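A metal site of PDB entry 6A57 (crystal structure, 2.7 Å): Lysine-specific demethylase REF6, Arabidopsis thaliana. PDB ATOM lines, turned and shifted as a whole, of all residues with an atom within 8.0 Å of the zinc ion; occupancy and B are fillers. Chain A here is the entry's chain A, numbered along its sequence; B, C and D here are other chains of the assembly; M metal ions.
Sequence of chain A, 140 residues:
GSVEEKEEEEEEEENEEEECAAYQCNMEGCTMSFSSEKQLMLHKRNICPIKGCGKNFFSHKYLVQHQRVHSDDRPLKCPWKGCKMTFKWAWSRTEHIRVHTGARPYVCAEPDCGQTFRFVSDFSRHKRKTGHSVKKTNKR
OP1 of DG 13 of chain B is in hydrogen-bond range of a ring nitrogen (ND1) of His 70 (2.6 Å). The backbone NH (N) of Gly 54 sits at hydrogen-bond distance from the backbone carbonyl oxygen (O) of Cys 48 (3.2 Å). The backbone NH (N) of Cys 48 is in hydrogen-bond range of the backbone carbonyl oxygen (O) of Lys 55 of chain A (3.1 Å). SG of Cys 48 sits close to NE2 of Gln 67, at 3.4 Å. ND1 of His 66 is in hydrogen-bond range of OP2 of DG 9 of chain C (2.9 Å).
Of the 20 residues printed, 4 come within 4 Å of the zinc ion.
NE2 of His 70 binds the zinc ion (2.0 Å). A ring nitrogen (NE2) of His 66 binds the zinc ion (2.0 Å). SG of Cys 53 is bound to the zinc ion. The zinc ion is bound by SG of Cys 48 (2.3 Å).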
ATOM      1  N   ILE A  47      18.407  18.686  17.571  1.00  0.00           N
ATOM      2  CA  ILE A  47      17.034  19.180  17.746  1.00  0.00           C
ATOM      3  C   ILE A  47      17.011  20.103  18.953  1.00  0.00           C
ATOM      4  O   ILE A  47      17.595  19.772  19.986  1.00  0.00           O
ATOM      5  CB  ILE A  47      16.020  18.040  17.971  1.00  0.00           C
ATOM      6  CG1 ILE A  47      16.088  17.007  16.830  1.00  0.00           C
ATOM      7  CG2 ILE A  47      14.603  18.604  18.067  1.00  0.00           C
ATOM      8  CD1 ILE A  47      15.256  15.765  17.060  1.00  0.00           C
ATOM      9  N   CYS A  48      16.329  21.244  18.827  1.00  0.00           N
ATOM     10  CA  CYS A  48      16.199  22.173  19.959  1.00  0.00           C
ATOM     11  C   CYS A  48      15.154  21.640  20.933  1.00  0.00           C
ATOM     12  O   CYS A  48      13.970  21.551  20.581  1.00  0.00           O
ATOM     13  CB  CYS A  48      15.809  23.584  19.503  1.00  0.00           C
ATOM     14  SG  CYS A  48      15.888  24.820  20.829  1.00  0.00           S
ATOM     15  N   PRO A  49      15.581  21.278  22.159  1.00  0.00           N
ATOM     16  CA  PRO A  49      14.651  20.678  23.111  1.00  0.00           C
ATOM     17  C   PRO A  49      13.664  21.660  23.750  1.00  0.00           C
ATOM     18  O   PRO A  49      12.631  21.221  24.241  1.00  0.00           O
ATOM     19  CB  PRO A  49      15.583  20.105  24.173  1.00  0.00           C
ATOM     20  CG  PRO A  49      16.734  21.058  24.188  1.00  0.00           C
ATOM     21  CD  PRO A  49      16.914  21.490  22.751  1.00  0.00           C
ATOM     22  N   ILE A  50      13.983  22.966  23.745  1.00  0.00           N
ATOM     23  CA  ILE A  50      13.105  23.988  24.340  1.00  0.00           C
ATOM     24  C   ILE A  50      11.654  23.749  23.916  1.00  0.00           C
ATOM     25  O   ILE A  50      11.392  23.448  22.758  1.00  0.00           O
ATOM     26  CB  ILE A  50      13.576  25.436  23.988  1.00  0.00           C
ATOM     27  CG1 ILE A  50      14.590  25.949  25.016  1.00  0.00           C
ATOM     28  CG2 ILE A  50      12.420  26.438  23.944  1.00  0.00           C
ATOM     29  CD1 ILE A  50      15.925  25.245  24.993  1.00  0.00           C
ATOM     30  N   LYS A  51      10.728  23.869  24.868  1.00  0.00           N
ATOM     31  CA  LYS A  51       9.329  23.541  24.613  1.00  0.00           C
ATOM     32  C   LYS A  51       8.748  24.554  23.630  1.00  0.00           C
ATOM     33  O   LYS A  51       8.981  25.753  23.752  1.00  0.00           O
ATOM     34  CB  LYS A  51       8.501  23.501  25.914  1.00  0.00           C
ATOM     35  CG  LYS A  51       7.326  22.536  25.841  1.00  0.00           C
ATOM     36  CD  LYS A  51       6.196  22.840  26.828  1.00  0.00           C
ATOM     37  CE  LYS A  51       6.527  22.433  28.259  1.00  0.00           C
ATOM     38  NZ  LYS A  51       6.610  20.955  28.473  1.00  0.00           N
ATOM     39  N   GLY A  52       8.025  24.068  22.620  1.00  0.00           N
ATOM     40  CA  GLY A  52       7.449  24.911  21.563  1.00  0.00           C
ATOM     41  C   GLY A  52       8.311  25.092  20.318  1.00  0.00           C
ATOM     42  O   GLY A  52       7.794  25.549  19.295  1.00  0.00           O
ATOM     43  N   CYS A  53       9.593  24.741  20.379  1.00  0.00           N
ATOM     44  CA  CYS A  53      10.518  24.875  19.253  1.00  0.00           C
ATOM     45  C   CYS A  53      10.587  23.558  18.457  1.00  0.00           C
ATOM     46  O   CYS A  53       9.806  23.371  17.518  1.00  0.00           O
ATOM     47  CB  CYS A  53      11.884  25.363  19.749  1.00  0.00           C
ATOM     48  SG  CYS A  53      13.102  25.601  18.443  1.00  0.00           S
ATOM     49  N   GLY A  54      11.480  22.652  18.852  1.00  0.00           N
ATOM     50  CA  GLY A  54      11.582  21.335  18.223  1.00  0.00           C
ATOM     51  C   GLY A  54      12.103  21.347  16.785  1.00  0.00           C
ATOM     52  O   GLY A  54      11.775  20.463  16.000  1.00  0.00           O
ATOM     53  N   LYS A  55      12.902  22.359  16.452  1.00  0.00           N
ATOM     54  CA  LYS A  55      13.444  22.504  15.101  1.00  0.00           C
ATOM     55  C   LYS A  55      14.644  21.598  14.912  1.00  0.00           C
ATOM     56  O   LYS A  55      15.455  21.459  15.822  1.00  0.00           O
ATOM     57  CB  LYS A  55      13.862  23.957  14.839  1.00  0.00           C
ATOM     58  CG  LYS A  55      12.711  24.923  14.660  1.00  0.00           C
ATOM     59  CD  LYS A  55      13.220  26.304  14.267  1.00  0.00           C
ATOM     60  CE  LYS A  55      12.094  27.217  13.816  1.00  0.00           C
ATOM     61  NZ  LYS A  55      12.597  28.361  13.011  1.00  0.00           N
ATOM     62  N   PHE A  57      18.233  20.909  12.901  1.00  0.00           N
ATOM     63  CA  PHE A  57      19.331  21.759  12.409  1.00  0.00           C
ATOM     64  C   PHE A  57      20.381  20.934  11.680  1.00  0.00           C
ATOM     65  O   PHE A  57      20.598  19.770  12.008  1.00  0.00           O
ATOM     66  CB  PHE A  57      19.953  22.544  13.568  1.00  0.00           C
ATOM     67  CG  PHE A  57      19.001  23.516  14.211  1.00  0.00           C
ATOM     68  CD1 PHE A  57      18.190  23.110  15.269  1.00  0.00           C
ATOM     69  CD2 PHE A  57      18.881  24.813  13.735  1.00  0.00           C
ATOM     70  CE1 PHE A  57      17.296  23.981  15.845  1.00  0.00           C
ATOM     71  CE2 PHE A  57      17.983  25.694  14.313  1.00  0.00           C
ATOM     72  CZ  PHE A  57      17.184  25.282  15.369  1.00  0.00           C
ATOM     73  N   LEU A  63      23.238  24.933  16.625  1.00  0.00           N
ATOM     74  CA  LEU A  63      22.272  24.653  17.717  1.00  0.00           C
ATOM     75  C   LEU A  63      22.526  25.499  18.977  1.00  0.00           C
ATOM     76  O   LEU A  63      21.597  25.928  19.628  1.00  0.00           O
ATOM     77  CB  LEU A  63      22.232  23.160  18.081  1.00  0.00           C
ATOM     78  CG  LEU A  63      20.854  22.538  18.308  1.00  0.00           C
ATOM     79  CD1 LEU A  63      20.991  21.105  18.811  1.00  0.00           C
ATOM     80  CD2 LEU A  63      19.980  23.338  19.271  1.00  0.00           C
ATOM     81  N   HIS A  66      21.748  29.127  17.769  1.00  0.00           N
ATOM     82  CA  HIS A  66      20.287  29.189  17.713  1.00  0.00           C
ATOM     83  C   HIS A  66      19.629  29.603  19.021  1.00  0.00           C
ATOM     84  O   HIS A  66      18.628  30.311  19.013  1.00  0.00           O
ATOM     85  CB  HIS A  66      19.710  27.822  17.286  1.00  0.00           C
ATOM     86  CG  HIS A  66      18.252  27.662  17.590  1.00  0.00           C
ATOM     87  ND1 HIS A  66      17.265  28.264  16.842  1.00  0.00           N
ATOM     88  CD2 HIS A  66      17.619  26.974  18.560  1.00  0.00           C
ATOM     89  CE1 HIS A  66      16.084  27.956  17.345  1.00  0.00           C
ATOM     90  NE2 HIS A  66      16.268  27.170  18.386  1.00  0.00           N
ATOM     91  N   GLN A  67      20.208  29.195  20.150  1.00  0.00           N
ATOM     92  CA  GLN A  67      19.597  29.434  21.458  1.00  0.00           C
ATOM     93  C   GLN A  67      19.328  30.905  21.769  1.00  0.00           C
ATOM     94  O   GLN A  67      18.507  31.194  22.647  1.00  0.00           O
ATOM     95  CB  GLN A  67      20.436  28.813  22.583  1.00  0.00           C
ATOM     96  CG  GLN A  67      20.550  27.279  22.555  1.00  0.00           C
ATOM     97  CD  GLN A  67      19.205  26.567  22.476  1.00  0.00           C
ATOM     98  OE1 GLN A  67      18.310  26.798  23.289  1.00  0.00           O
ATOM     99  NE2 GLN A  67      19.067  25.672  21.489  1.00  0.00           N
ATOM    100  N   ARG A  68      19.994  31.825  21.065  1.00  0.00           N
ATOM    101  CA  ARG A  68      19.766  33.259  21.265  1.00  0.00           C
ATOM    102  C   ARG A  68      18.353  33.740  20.929  1.00  0.00           C
ATOM    103  O   ARG A  68      17.908  34.747  21.476  1.00  0.00           O
ATOM    104  CB  ARG A  68      20.788  34.099  20.490  1.00  0.00           C
ATOM    105  CG  ARG A  68      20.567  34.149  18.986  1.00  0.00           C
ATOM    106  CD  ARG A  68      21.724  34.841  18.301  1.00  0.00           C
ATOM    107  NE  ARG A  68      22.931  34.019  18.299  1.00  0.00           N
ATOM    108  CZ  ARG A  68      24.119  34.419  17.841  1.00  0.00           C
ATOM    109  NH1 ARG A  68      24.295  35.636  17.325  1.00  0.00           N
ATOM    110  NH2 ARG A  68      25.158  33.580  17.895  1.00  0.00           N
ATOM    111  N   VAL A  69      17.639  33.020  20.042  1.00  0.00           N
ATOM    112  CA  VAL A  69      16.239  33.351  19.754  1.00  0.00           C
ATOM    113  C   VAL A  69      15.352  33.143  20.981  1.00  0.00           C
ATOM    114  O   VAL A  69      14.306  33.788  21.117  1.00  0.00           O
ATOM    115  CB  VAL A  69      15.634  32.565  18.562  1.00  0.00           C
ATOM    116  CG1 VAL A  69      16.427  32.813  17.282  1.00  0.00           C
ATOM    117  CG2 VAL A  69      15.520  31.069  18.846  1.00  0.00           C
ATOM    118  N   HIS A  70      15.756  32.235  21.857  1.00  0.00           N
ATOM    119  CA  HIS A  70      15.037  31.973  23.094  1.00  0.00           C
ATOM    120  C   HIS A  70      15.407  32.957  24.215  1.00  0.00           C
ATOM    121  O   HIS A  70      14.590  33.227  25.080  1.00  0.00           O
ATOM    122  CB  HIS A  70      15.202  30.510  23.489  1.00  0.00           C
ATOM    123  CG  HIS A  70      14.742  29.564  22.426  1.00  0.00           C
ATOM    124  ND1 HIS A  70      13.431  29.508  21.994  1.00  0.00           N
ATOM    125  CD2 HIS A  70      15.419  28.643  21.687  1.00  0.00           C
ATOM    126  CE1 HIS A  70      13.319  28.607  21.033  1.00  0.00           C
ATOM    127  NE2 HIS A  70      14.507  28.056  20.841  1.00  0.00           N
ATOM    128  P    DA B  12       9.376  27.581  29.120  1.00  0.00           P
ATOM    129  OP1  DA B  12      10.651  26.866  28.852  1.00  0.00           O
ATOM    130  OP2  DA B  12       9.282  28.555  30.240  1.00  0.00           O
ATOM    131  O5'  DA B  12       8.942  28.334  27.781  1.00  0.00           O
ATOM    132  C5'  DA B  12       9.040  27.698  26.492  1.00  0.00           C
ATOM    133  C4'  DA B  12       8.572  28.662  25.427  1.00  0.00           C
ATOM    134  O4'  DA B  12       7.198  29.061  25.687  1.00  0.00           O
ATOM    135  C3'  DA B  12       9.385  29.961  25.367  1.00  0.00           C
ATOM    136  O3'  DA B  12       9.783  30.219  24.016  1.00  0.00           O
ATOM    137  C2'  DA B  12       8.444  31.007  25.953  1.00  0.00           C
ATOM    138  C1'  DA B  12       7.087  30.466  25.564  1.00  0.00           C
ATOM    139  N9   DA B  12       5.989  30.912  26.424  1.00  0.00           N
ATOM    140  C8   DA B  12       5.907  30.826  27.789  1.00  0.00           C
ATOM    141  N7   DA B  12       4.791  31.310  28.280  1.00  0.00           N
ATOM    142  C5   DA B  12       4.102  31.767  27.161  1.00  0.00           C
ATOM    143  C6   DA B  12       2.860  32.407  27.003  1.00  0.00           C
ATOM    144  N6   DA B  12       2.054  32.704  28.021  1.00  0.00           N
ATOM    145  N1   DA B  12       2.484  32.735  25.756  1.00  0.00           N
ATOM    146  C2   DA B  12       3.288  32.438  24.728  1.00  0.00           C
ATOM    147  N3   DA B  12       4.479  31.831  24.745  1.00  0.00           N
ATOM    148  C4   DA B  12       4.838  31.528  26.006  1.00  0.00           C
ATOM    149  P    DG B  13      10.878  31.334  23.696  1.00  0.00           P
ATOM    150  OP1  DG B  13      11.402  31.075  22.319  1.00  0.00           O
ATOM    151  OP2  DG B  13      11.820  31.439  24.847  1.00  0.00           O
ATOM    152  O5'  DG B  13      10.029  32.672  23.680  1.00  0.00           O
ATOM    153  C5'  DG B  13       8.941  32.840  22.764  1.00  0.00           C
ATOM    154  C4'  DG B  13       8.195  34.119  23.073  1.00  0.00           C
ATOM    155  O4'  DG B  13       7.231  33.886  24.127  1.00  0.00           O
ATOM    156  C3'  DG B  13       9.081  35.281  23.550  1.00  0.00           C
ATOM    157  O3'  DG B  13       8.710  36.498  22.904  1.00  0.00           O
ATOM    158  C2'  DG B  13       8.686  35.443  25.012  1.00  0.00           C
ATOM    159  C1'  DG B  13       7.225  35.067  24.904  1.00  0.00           C
ATOM    160  N9   DG B  13       6.517  34.839  26.153  1.00  0.00           N
ATOM    161  C8   DG B  13       6.983  34.235  27.295  1.00  0.00           C
ATOM    162  N7   DG B  13       6.122  34.267  28.271  1.00  0.00           N
ATOM    163  C5   DG B  13       5.037  34.968  27.758  1.00  0.00           C
ATOM    164  C6   DG B  13       3.804  35.329  28.349  1.00  0.00           C
ATOM    165  O6   DG B  13       3.404  35.095  29.499  1.00  0.00           O
ATOM    166  N1   DG B  13       2.991  36.025  27.460  1.00  0.00           N
ATOM    167  C2   DG B  13       3.322  36.349  26.175  1.00  0.00           C
ATOM    168  N2   DG B  13       2.408  37.033  25.462  1.00  0.00           N
ATOM    169  N3   DG B  13       4.473  36.022  25.609  1.00  0.00           N
ATOM    170  C4   DG B  13       5.275  35.339  26.451  1.00  0.00           C
ATOM    171  P    DG C   9      16.801  29.481  13.178  1.00  0.00           P
ATOM    172  OP1  DG C   9      15.363  29.343  13.520  1.00  0.00           O
ATOM    173  OP2  DG C   9      17.818  29.525  14.252  1.00  0.00           O
ATOM    174  O5'  DG C   9      17.125  28.303  12.160  1.00  0.00           O
ATOM    175  C5'  DG C   9      16.142  27.855  11.203  1.00  0.00           C
ATOM    176  C4'  DG C   9      16.817  27.432   9.922  1.00  0.00           C
ATOM    177  O4'  DG C   9      17.362  28.595   9.244  1.00  0.00           O
ATOM    178  C3'  DG C   9      17.988  26.455  10.067  1.00  0.00           C
ATOM    179  O3'  DG C   9      17.884  25.518   8.990  1.00  0.00           O
ATOM    180  C2'  DG C   9      19.207  27.349   9.965  1.00  0.00           C
ATOM    181  C1'  DG C   9      18.749  28.411   8.987  1.00  0.00           C
ATOM    182  N9   DG C   9      19.381  29.716   9.097  1.00  0.00           N
ATOM    183  C8   DG C   9      19.640  30.408  10.253  1.00  0.00           C
ATOM    184  N7   DG C   9      20.180  31.576  10.043  1.00  0.00           N
ATOM    185  C5   DG C   9      20.265  31.676   8.657  1.00  0.00           C
ATOM    186  C6   DG C   9      20.770  32.716   7.844  1.00  0.00           C
ATOM    187  O6   DG C   9      21.248  33.808   8.185  1.00  0.00           O
ATOM    188  N1   DG C   9      20.670  32.395   6.487  1.00  0.00           N
ATOM    189  C2   DG C   9      20.146  31.223   5.995  1.00  0.00           C
ATOM    190  N2   DG C   9      20.142  31.099   4.658  1.00  0.00           N
ATOM    191  N3   DG C   9      19.686  30.247   6.745  1.00  0.00           N
ATOM    192  C4   DG C   9      19.771  30.536   8.062  1.00  0.00           C
ATOM    193  N   LYS D  55      10.554  22.166  11.919  1.00  0.00           N
ATOM    194  CA  LYS D  55      10.121  21.680  13.228  1.00  0.00           C
ATOM    195  C   LYS D  55       9.664  20.238  13.132  1.00  0.00           C
ATOM    196  O   LYS D  55       9.014  19.865  12.160  1.00  0.00           O
ATOM    197  CB  LYS D  55       8.972  22.539  13.772  1.00  0.00           C
ATOM    198  CG  LYS D  55       9.381  23.920  14.246  1.00  0.00           C
ATOM    199  CD  LYS D  55       8.204  24.642  14.885  1.00  0.00           C
ATOM    200  CE  LYS D  55       8.642  25.907  15.610  1.00  0.00           C
ATOM    201  NZ  LYS D  55       7.636  26.354  16.608  1.00  0.00           N
HETATM  202 ZN    ZN M   1      14.826  26.498  19.633  1.00  0.00          ZN
